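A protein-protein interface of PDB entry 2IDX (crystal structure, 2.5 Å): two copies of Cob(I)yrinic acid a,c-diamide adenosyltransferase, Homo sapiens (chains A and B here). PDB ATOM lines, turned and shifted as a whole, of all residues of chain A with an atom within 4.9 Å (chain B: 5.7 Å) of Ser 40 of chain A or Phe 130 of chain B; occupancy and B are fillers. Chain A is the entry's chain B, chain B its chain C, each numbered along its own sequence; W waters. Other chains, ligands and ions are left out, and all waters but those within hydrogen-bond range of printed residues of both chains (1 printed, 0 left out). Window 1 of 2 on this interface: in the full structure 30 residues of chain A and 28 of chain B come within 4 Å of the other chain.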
ATOM      1  N   ASP A  36      -2.924  31.216 -25.306  1.00  0.00           N
ATOM      2  CA  ASP A  36      -3.331  29.946 -25.935  1.00  0.00           C
ATOM      3  C   ASP A  36      -3.841  29.003 -24.849  1.00  0.00           C
ATOM      4  O   ASP A  36      -4.918  28.420 -24.970  1.00  0.00           O
ATOM      5  CB  ASP A  36      -2.169  29.315 -26.721  1.00  0.00           C
ATOM      6  CG  ASP A  36      -2.500  27.935 -27.299  1.00  0.00           C
ATOM      7  OD1 ASP A  36      -3.711  27.575 -27.484  1.00  0.00           O
ATOM      8  OD2 ASP A  36      -1.516  27.200 -27.581  1.00  0.00           O
ATOM      9  N   GLU A  37      -3.085  28.894 -23.764  1.00  0.00           N
ATOM     10  CA  GLU A  37      -3.468  28.009 -22.666  1.00  0.00           C
ATOM     11  C   GLU A  37      -4.913  28.298 -22.230  1.00  0.00           C
ATOM     12  O   GLU A  37      -5.707  27.377 -22.082  1.00  0.00           O
ATOM     13  CB  GLU A  37      -2.486  28.120 -21.506  1.00  0.00           C
ATOM     14  CG  GLU A  37      -2.578  26.991 -20.544  1.00  0.00           C
ATOM     15  CD  GLU A  37      -1.532  27.083 -19.446  1.00  0.00           C
ATOM     16  OE1 GLU A  37      -0.430  27.645 -19.689  1.00  0.00           O
ATOM     17  OE2 GLU A  37      -1.813  26.619 -18.318  1.00  0.00           O
ATOM     18  N   LEU A  38      -5.240  29.583 -22.090  1.00  0.00           N
ATOM     19  CA  LEU A  38      -6.565  30.023 -21.704  1.00  0.00           C
ATOM     20  C   LEU A  38      -7.580  29.573 -22.716  1.00  0.00           C
ATOM     21  O   LEU A  38      -8.670  29.155 -22.347  1.00  0.00           O
ATOM     22  CB  LEU A  38      -6.631  31.547 -21.572  1.00  0.00           C
ATOM     23  CG  LEU A  38      -8.025  32.201 -21.356  1.00  0.00           C
ATOM     24  CD1 LEU A  38      -8.755  31.670 -20.113  1.00  0.00           C
ATOM     25  CD2 LEU A  38      -7.942  33.720 -21.287  1.00  0.00           C
ATOM     26  N   SER A  39      -7.242  29.665 -23.999  1.00  0.00           N
ATOM     27  CA  SER A  39      -8.233  29.364 -25.026  1.00  0.00           C
ATOM     28  C   SER A  39      -8.507  27.871 -25.025  1.00  0.00           C
ATOM     29  O   SER A  39      -9.635  27.442 -25.190  1.00  0.00           O
ATOM     30  CB  SER A  39      -7.765  29.838 -26.399  1.00  0.00           C
ATOM     31  OG  SER A  39      -8.738  29.524 -27.366  1.00  0.00           O
ATOM     32  N   SER A  40      -7.459  27.090 -24.811  1.00  0.00           N
ATOM     33  CA  SER A  40      -7.562  25.657 -24.623  1.00  0.00           C
ATOM     34  C   SER A  40      -8.368  25.232 -23.410  1.00  0.00           C
ATOM     35  O   SER A  40      -9.018  24.175 -23.430  1.00  0.00           O
ATOM     36  CB  SER A  40      -6.164  25.074 -24.471  1.00  0.00           C
ATOM     37  OG  SER A  40      -5.725  24.587 -25.718  1.00  0.00           O
ATOM     38  N   ALA A  41      -8.300  26.020 -22.342  1.00  0.00           N
ATOM     39  CA  ALA A  41      -9.023  25.666 -21.142  1.00  0.00           C
ATOM     40  C   ALA A  41     -10.505  25.886 -21.422  1.00  0.00           C
ATOM     41  O   ALA A  41     -11.326  25.013 -21.141  1.00  0.00           O
ATOM     42  CB  ALA A  41      -8.537  26.481 -19.948  1.00  0.00           C
ATOM     43  N   ILE A  42     -10.833  27.026 -22.028  1.00  0.00           N
ATOM     44  CA  ILE A  42     -12.186  27.277 -22.494  1.00  0.00           C
ATOM     45  C   ILE A  42     -12.688  26.176 -23.451  1.00  0.00           C
ATOM     46  O   ILE A  42     -13.831  25.708 -23.327  1.00  0.00           O
ATOM     47  CB  ILE A  42     -12.300  28.671 -23.138  1.00  0.00           C
ATOM     48  CG1 ILE A  42     -12.273  29.745 -22.043  1.00  0.00           C
ATOM     49  CG2 ILE A  42     -13.547  28.768 -23.997  1.00  0.00           C
ATOM     50  CD1 ILE A  42     -11.692  31.041 -22.498  1.00  0.00           C
ATOM     51  N   GLY A  43     -11.824  25.747 -24.368  1.00  0.00           N
ATOM     52  CA  GLY A  43     -12.131  24.623 -25.240  1.00  0.00           C
ATOM     53  C   GLY A  43     -12.562  23.383 -24.460  1.00  0.00           C
ATOM     54  O   GLY A  43     -13.554  22.728 -24.803  1.00  0.00           O
ATOM     55  N   PHE A  44     -11.845  23.061 -23.391  1.00  0.00           N
ATOM     56  CA  PHE A  44     -12.236  21.897 -22.620  1.00  0.00           C
ATOM     57  C   PHE A  44     -13.557  22.108 -21.879  1.00  0.00           C
ATOM     58  O   PHE A  44     -14.413  21.232 -21.896  1.00  0.00           O
ATOM     59  CB  PHE A  44     -11.148  21.412 -21.655  1.00  0.00           C
ATOM     60  CG  PHE A  44     -11.550  20.171 -20.913  1.00  0.00           C
ATOM     61  CD1 PHE A  44     -11.470  18.916 -21.539  1.00  0.00           C
ATOM     62  CD2 PHE A  44     -12.060  20.254 -19.608  1.00  0.00           C
ATOM     63  CE1 PHE A  44     -11.860  17.759 -20.880  1.00  0.00           C
ATOM     64  CE2 PHE A  44     -12.464  19.097 -18.920  1.00  0.00           C
ATOM     65  CZ  PHE A  44     -12.370  17.838 -19.558  1.00  0.00           C
ATOM     66  N   PHE A 130     -11.500  27.481 -13.103  1.00  0.00           N
ATOM     67  CA  PHE A 130     -10.173  27.187 -13.540  1.00  0.00           C
ATOM     68  C   PHE A 130      -9.798  28.127 -14.700  1.00  0.00           C
ATOM     69  O   PHE A 130      -8.768  28.814 -14.635  1.00  0.00           O
ATOM     70  CB  PHE A 130     -10.059  25.697 -13.939  1.00  0.00           C
ATOM     71  CG  PHE A 130      -8.678  25.301 -14.347  1.00  0.00           C
ATOM     72  CD1 PHE A 130      -7.622  25.355 -13.421  1.00  0.00           C
ATOM     73  CD2 PHE A 130      -8.410  24.920 -15.646  1.00  0.00           C
ATOM     74  CE1 PHE A 130      -6.305  25.021 -13.812  1.00  0.00           C
ATOM     75  CE2 PHE A 130      -7.110  24.575 -16.035  1.00  0.00           C
ATOM     76  CZ  PHE A 130      -6.062  24.625 -15.119  1.00  0.00           C
ATOM     77  N   ALA B  41      -1.032  16.441 -17.192  1.00  0.00           N
ATOM     78  CA  ALA B  41      -2.115  16.827 -18.085  1.00  0.00           C
ATOM     79  C   ALA B  41      -2.365  15.674 -19.044  1.00  0.00           C
ATOM     80  O   ALA B  41      -3.510  15.278 -19.245  1.00  0.00           O
ATOM     81  CB  ALA B  41      -1.766  18.112 -18.842  1.00  0.00           C
ATOM     82  N   PRO B 119      -9.137  25.348 -30.203  1.00  0.00           N
ATOM     83  CA  PRO B 119      -9.239  24.228 -29.278  1.00  0.00           C
ATOM     84  C   PRO B 119     -10.694  23.780 -29.127  1.00  0.00           C
ATOM     85  O   PRO B 119     -11.532  24.522 -28.619  1.00  0.00           O
ATOM     86  CB  PRO B 119      -8.709  24.815 -27.976  1.00  0.00           C
ATOM     87  CG  PRO B 119      -7.787  25.861 -28.398  1.00  0.00           C
ATOM     88  CD  PRO B 119      -8.436  26.485 -29.575  1.00  0.00           C
ATOM     89  N   SER B 125      -9.868  15.369 -27.709  1.00  0.00           N
ATOM     90  CA  SER B 125      -9.273  16.382 -28.550  1.00  0.00           C
ATOM     91  C   SER B 125      -9.047  17.706 -27.787  1.00  0.00           C
ATOM     92  O   SER B 125      -8.010  18.372 -27.917  1.00  0.00           O
ATOM     93  CB  SER B 125     -10.190  16.610 -29.741  1.00  0.00           C
ATOM     94  OG  SER B 125      -9.635  17.536 -30.623  1.00  0.00           O
ATOM     95  N   SER B 126     -10.007  18.090 -26.970  1.00  0.00           N
ATOM     96  CA  SER B 126      -9.821  19.316 -26.238  1.00  0.00           C
ATOM     97  C   SER B 126      -8.813  19.131 -25.141  1.00  0.00           C
ATOM     98  O   SER B 126      -8.023  20.039 -24.895  1.00  0.00           O
ATOM     99  CB  SER B 126     -11.136  19.852 -25.705  1.00  0.00           C
ATOM    100  OG  SER B 126     -11.962  20.160 -26.825  1.00  0.00           O
ATOM    101  N   ALA B 127      -8.807  17.961 -24.505  1.00  0.00           N
ATOM    102  CA  ALA B 127      -7.798  17.705 -23.462  1.00  0.00           C
ATOM    103  C   ALA B 127      -6.389  17.778 -24.080  1.00  0.00           C
ATOM    104  O   ALA B 127      -5.453  18.347 -23.481  1.00  0.00           O
ATOM    105  CB  ALA B 127      -8.034  16.392 -22.755  1.00  0.00           C
ATOM    106  N   LEU B 128      -6.280  17.276 -25.304  1.00  0.00           N
ATOM    107  CA  LEU B 128      -5.012  17.286 -26.033  1.00  0.00           C
ATOM    108  C   LEU B 128      -4.556  18.670 -26.425  1.00  0.00           C
ATOM    109  O   LEU B 128      -3.352  18.939 -26.437  1.00  0.00           O
ATOM    110  CB  LEU B 128      -5.044  16.349 -27.239  1.00  0.00           C
ATOM    111  CG  LEU B 128      -5.020  14.880 -26.769  1.00  0.00           C
ATOM    112  CD1 LEU B 128      -5.403  13.864 -27.847  1.00  0.00           C
ATOM    113  CD2 LEU B 128      -3.684  14.515 -26.140  1.00  0.00           C
ATOM    114  N   HIS B 129      -5.507  19.551 -26.736  1.00  0.00           N
ATOM    115  CA  HIS B 129      -5.162  20.930 -27.073  1.00  0.00           C
ATOM    116  C   HIS B 129      -4.665  21.697 -25.840  1.00  0.00           C
ATOM    117  O   HIS B 129      -3.745  22.551 -25.936  1.00  0.00           O
ATOM    118  CB  HIS B 129      -6.333  21.635 -27.714  1.00  0.00           C
ATOM    119  CG  HIS B 129      -6.432  21.404 -29.183  1.00  0.00           C
ATOM    120  ND1 HIS B 129      -7.428  20.643 -29.753  1.00  0.00           N
ATOM    121  CD2 HIS B 129      -5.643  21.816 -30.201  1.00  0.00           C
ATOM    122  CE1 HIS B 129      -7.264  20.617 -31.062  1.00  0.00           C
ATOM    123  NE2 HIS B 129      -6.187  21.324 -31.360  1.00  0.00           N
ATOM    124  N   PHE B 130      -5.274  21.392 -24.689  1.00  0.00           N
ATOM    125  CA  PHE B 130      -4.796  21.929 -23.426  1.00  0.00           C
ATOM    126  C   PHE B 130      -3.380  21.430 -23.168  1.00  0.00           C
ATOM    127  O   PHE B 130      -2.472  22.246 -22.900  1.00  0.00           O
ATOM    128  CB  PHE B 130      -5.720  21.554 -22.259  1.00  0.00           C
ATOM    129  CG  PHE B 130      -5.260  22.080 -20.907  1.00  0.00           C
ATOM    130  CD1 PHE B 130      -5.296  23.445 -20.624  1.00  0.00           C
ATOM    131  CD2 PHE B 130      -4.828  21.194 -19.915  1.00  0.00           C
ATOM    132  CE1 PHE B 130      -4.878  23.919 -19.396  1.00  0.00           C
ATOM    133  CE2 PHE B 130      -4.422  21.655 -18.670  1.00  0.00           C
ATOM    134  CZ  PHE B 130      -4.431  23.015 -18.406  1.00  0.00           C
ATOM    135  N   CYS B 131      -3.186  20.108 -23.259  1.00  0.00           N
ATOM    136  CA  CYS B 131      -1.843  19.498 -23.157  1.00  0.00           C
ATOM    137  C   CYS B 131      -0.826  20.232 -24.049  1.00  0.00           C
ATOM    138  O   CYS B 131       0.249  20.589 -23.586  1.00  0.00           O
ATOM    139  CB  CYS B 131      -1.869  18.006 -23.514  1.00  0.00           C
ATOM    140  SG  CYS B 131      -2.724  16.912 -22.348  1.00  0.00           S
ATOM    141  N   ARG B 132      -1.189  20.480 -25.303  1.00  0.00           N
ATOM    142  CA  ARG B 132      -0.317  21.166 -26.236  1.00  0.00           C
ATOM    143  C   ARG B 132       0.093  22.540 -25.691  1.00  0.00           C
ATOM    144  O   ARG B 132       1.257  22.934 -25.764  1.00  0.00           O
ATOM    145  CB  ARG B 132      -0.981  21.292 -27.625  1.00  0.00           C
ATOM    146  CG  ARG B 132      -0.124  21.991 -28.668  1.00  0.00           C
ATOM    147  CD  ARG B 132      -0.839  22.188 -30.005  1.00  0.00           C
ATOM    148  NE  ARG B 132      -0.805  23.612 -30.383  1.00  0.00           N
ATOM    149  CZ  ARG B 132       0.022  24.161 -31.281  1.00  0.00           C
ATOM    150  NH1 ARG B 132       0.886  23.422 -31.958  1.00  0.00           N
ATOM    151  NH2 ARG B 132      -0.018  25.458 -31.501  1.00  0.00           N
ATOM    152  N   ALA B 133      -0.857  23.252 -25.112  1.00  0.00           N
ATOM    153  CA  ALA B 133      -0.563  24.546 -24.564  1.00  0.00           C
ATOM    154  C   ALA B 133       0.424  24.371 -23.415  1.00  0.00           C
ATOM    155  O   ALA B 133       1.421  25.097 -23.342  1.00  0.00           O
ATOM    156  CB  ALA B 133      -1.827  25.232 -24.113  1.00  0.00           C
ATOM    157  N   VAL B 134       0.166  23.376 -22.554  1.00  0.00           N
ATOM    158  CA  VAL B 134       1.013  23.150 -21.383  1.00  0.00           C
ATOM    159  C   VAL B 134       2.419  22.759 -21.841  1.00  0.00           C
ATOM    160  O   VAL B 134       3.415  23.159 -21.227  1.00  0.00           O
ATOM    161  CB  VAL B 134       0.413  22.084 -20.432  1.00  0.00           C
ATOM    162  CG1 VAL B 134       1.368  21.751 -19.257  1.00  0.00           C
ATOM    163  CG2 VAL B 134      -0.962  22.520 -19.898  1.00  0.00           C
ATOM    164  N   CYS B 135       2.485  21.990 -22.931  1.00  0.00           N
ATOM    165  CA  CYS B 135       3.737  21.535 -23.498  1.00  0.00           C
ATOM    166  C   CYS B 135       4.592  22.706 -23.969  1.00  0.00           C
ATOM    167  O   CYS B 135       5.788  22.742 -23.760  1.00  0.00           O
ATOM    168  CB  CYS B 135       3.460  20.588 -24.666  1.00  0.00           C
ATOM    169  SG  CYS B 135       4.974  19.920 -25.448  1.00  0.00           S
HETATM  170  O   HOH W   1      -3.377  24.620 -28.001  1.00  0.00           O
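The side-chain hydroxyl (OG) of Ser 40 of chain A lies within hydrogen-bond range of the backbone NH (N) of Phe 130 of chain B. The side-chain hydroxyl (OG) of Ser 40 of chain A lies within hydrogen-bond range of the backbone carbonyl oxygen (O) of His 129 of chain B, 2.8 Å away.
Water W1 lies within hydrogen-bond range of the backbone carbonyl oxygen (O) of His 129 of chain B (2.9 Å), the side-chain carboxylate (OD1) of Asp 36 of chain A (3.0 Å) and the side-chain hydroxyl (OG) of Ser 40 of chain A (3.3 Å).
Of the printed residues of chain B, Ser 39 of chain A touches Pro 119. Ser 40 of chain A touches three residues of chain B. Of the printed residues of chain A, Pro 119 of chain B touches Ser 39, Ser 40 and Gly 43. Printed residues of chain A within 4 Å of Ser 126 of chain B: Gly 43 and Phe 44. Leu 128 of chain B touches none of the printed residues of chain A. Of the printed residues of chain A, Phe 130 of chain B touches Ser 40 and Phe 130. Arg 132 of chain B touches none of the printed residues of chain A. The nearest printed residue of chain A that does not touch Phe 130 of chain B is Glu 37 of chain A (4.01 Å). The nearest printed residue of chain A that does not touch His 129 of chain B is Asp 36 of chain A (5.3 Å).
Phe 130 of chain B touches its own counterpart, Phe 130 of chain A. Of the 10 pairs that touch across the chains among the printed residues, 1 has its exchanged pair printed and touching as well.
Hydrophobic or aromatic side chains of chain A that line the printed part of chain B: Phe 130. Of the 13 printed residues of chain B, 5 touch a printed residue of chain A. Printed residues of chain B that touch a printed residue of chain A: Pro 119, Ser 126, His 129, Phe 130 and Ala 133. Among the printed residues, no Asp or Glu carboxylate lies within 4 Å of a Lys or Arg side-chain nitrogen of the other chain.
Asp 36 of chain A touches Ala 133 of chain B. CA of Glu 37 of chain A touches CB of Ala 133 of chain B (3.5 Å). CD of Pro 119 of chain B touches OG of Ser 39 of chain A (3.8 Å). Pro 119 of chain B touches Ser 40 of chain A. Pro 119 of chain B touches Gly 43 of chain A (O to CA, 3.4 Å). Ser 126 of chain B touches Gly 43 of chain A. Phe 44 of chain A touches Ser 126 of chain B. Phe 130 of chain B touches Phe 130 of chain A.
The backbone carbonyl oxygen (O) of Ser 125 of chain B lies within hydrogen-bond range of a ring nitrogen (ND1) of His 129 of chain B (3.0 Å).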
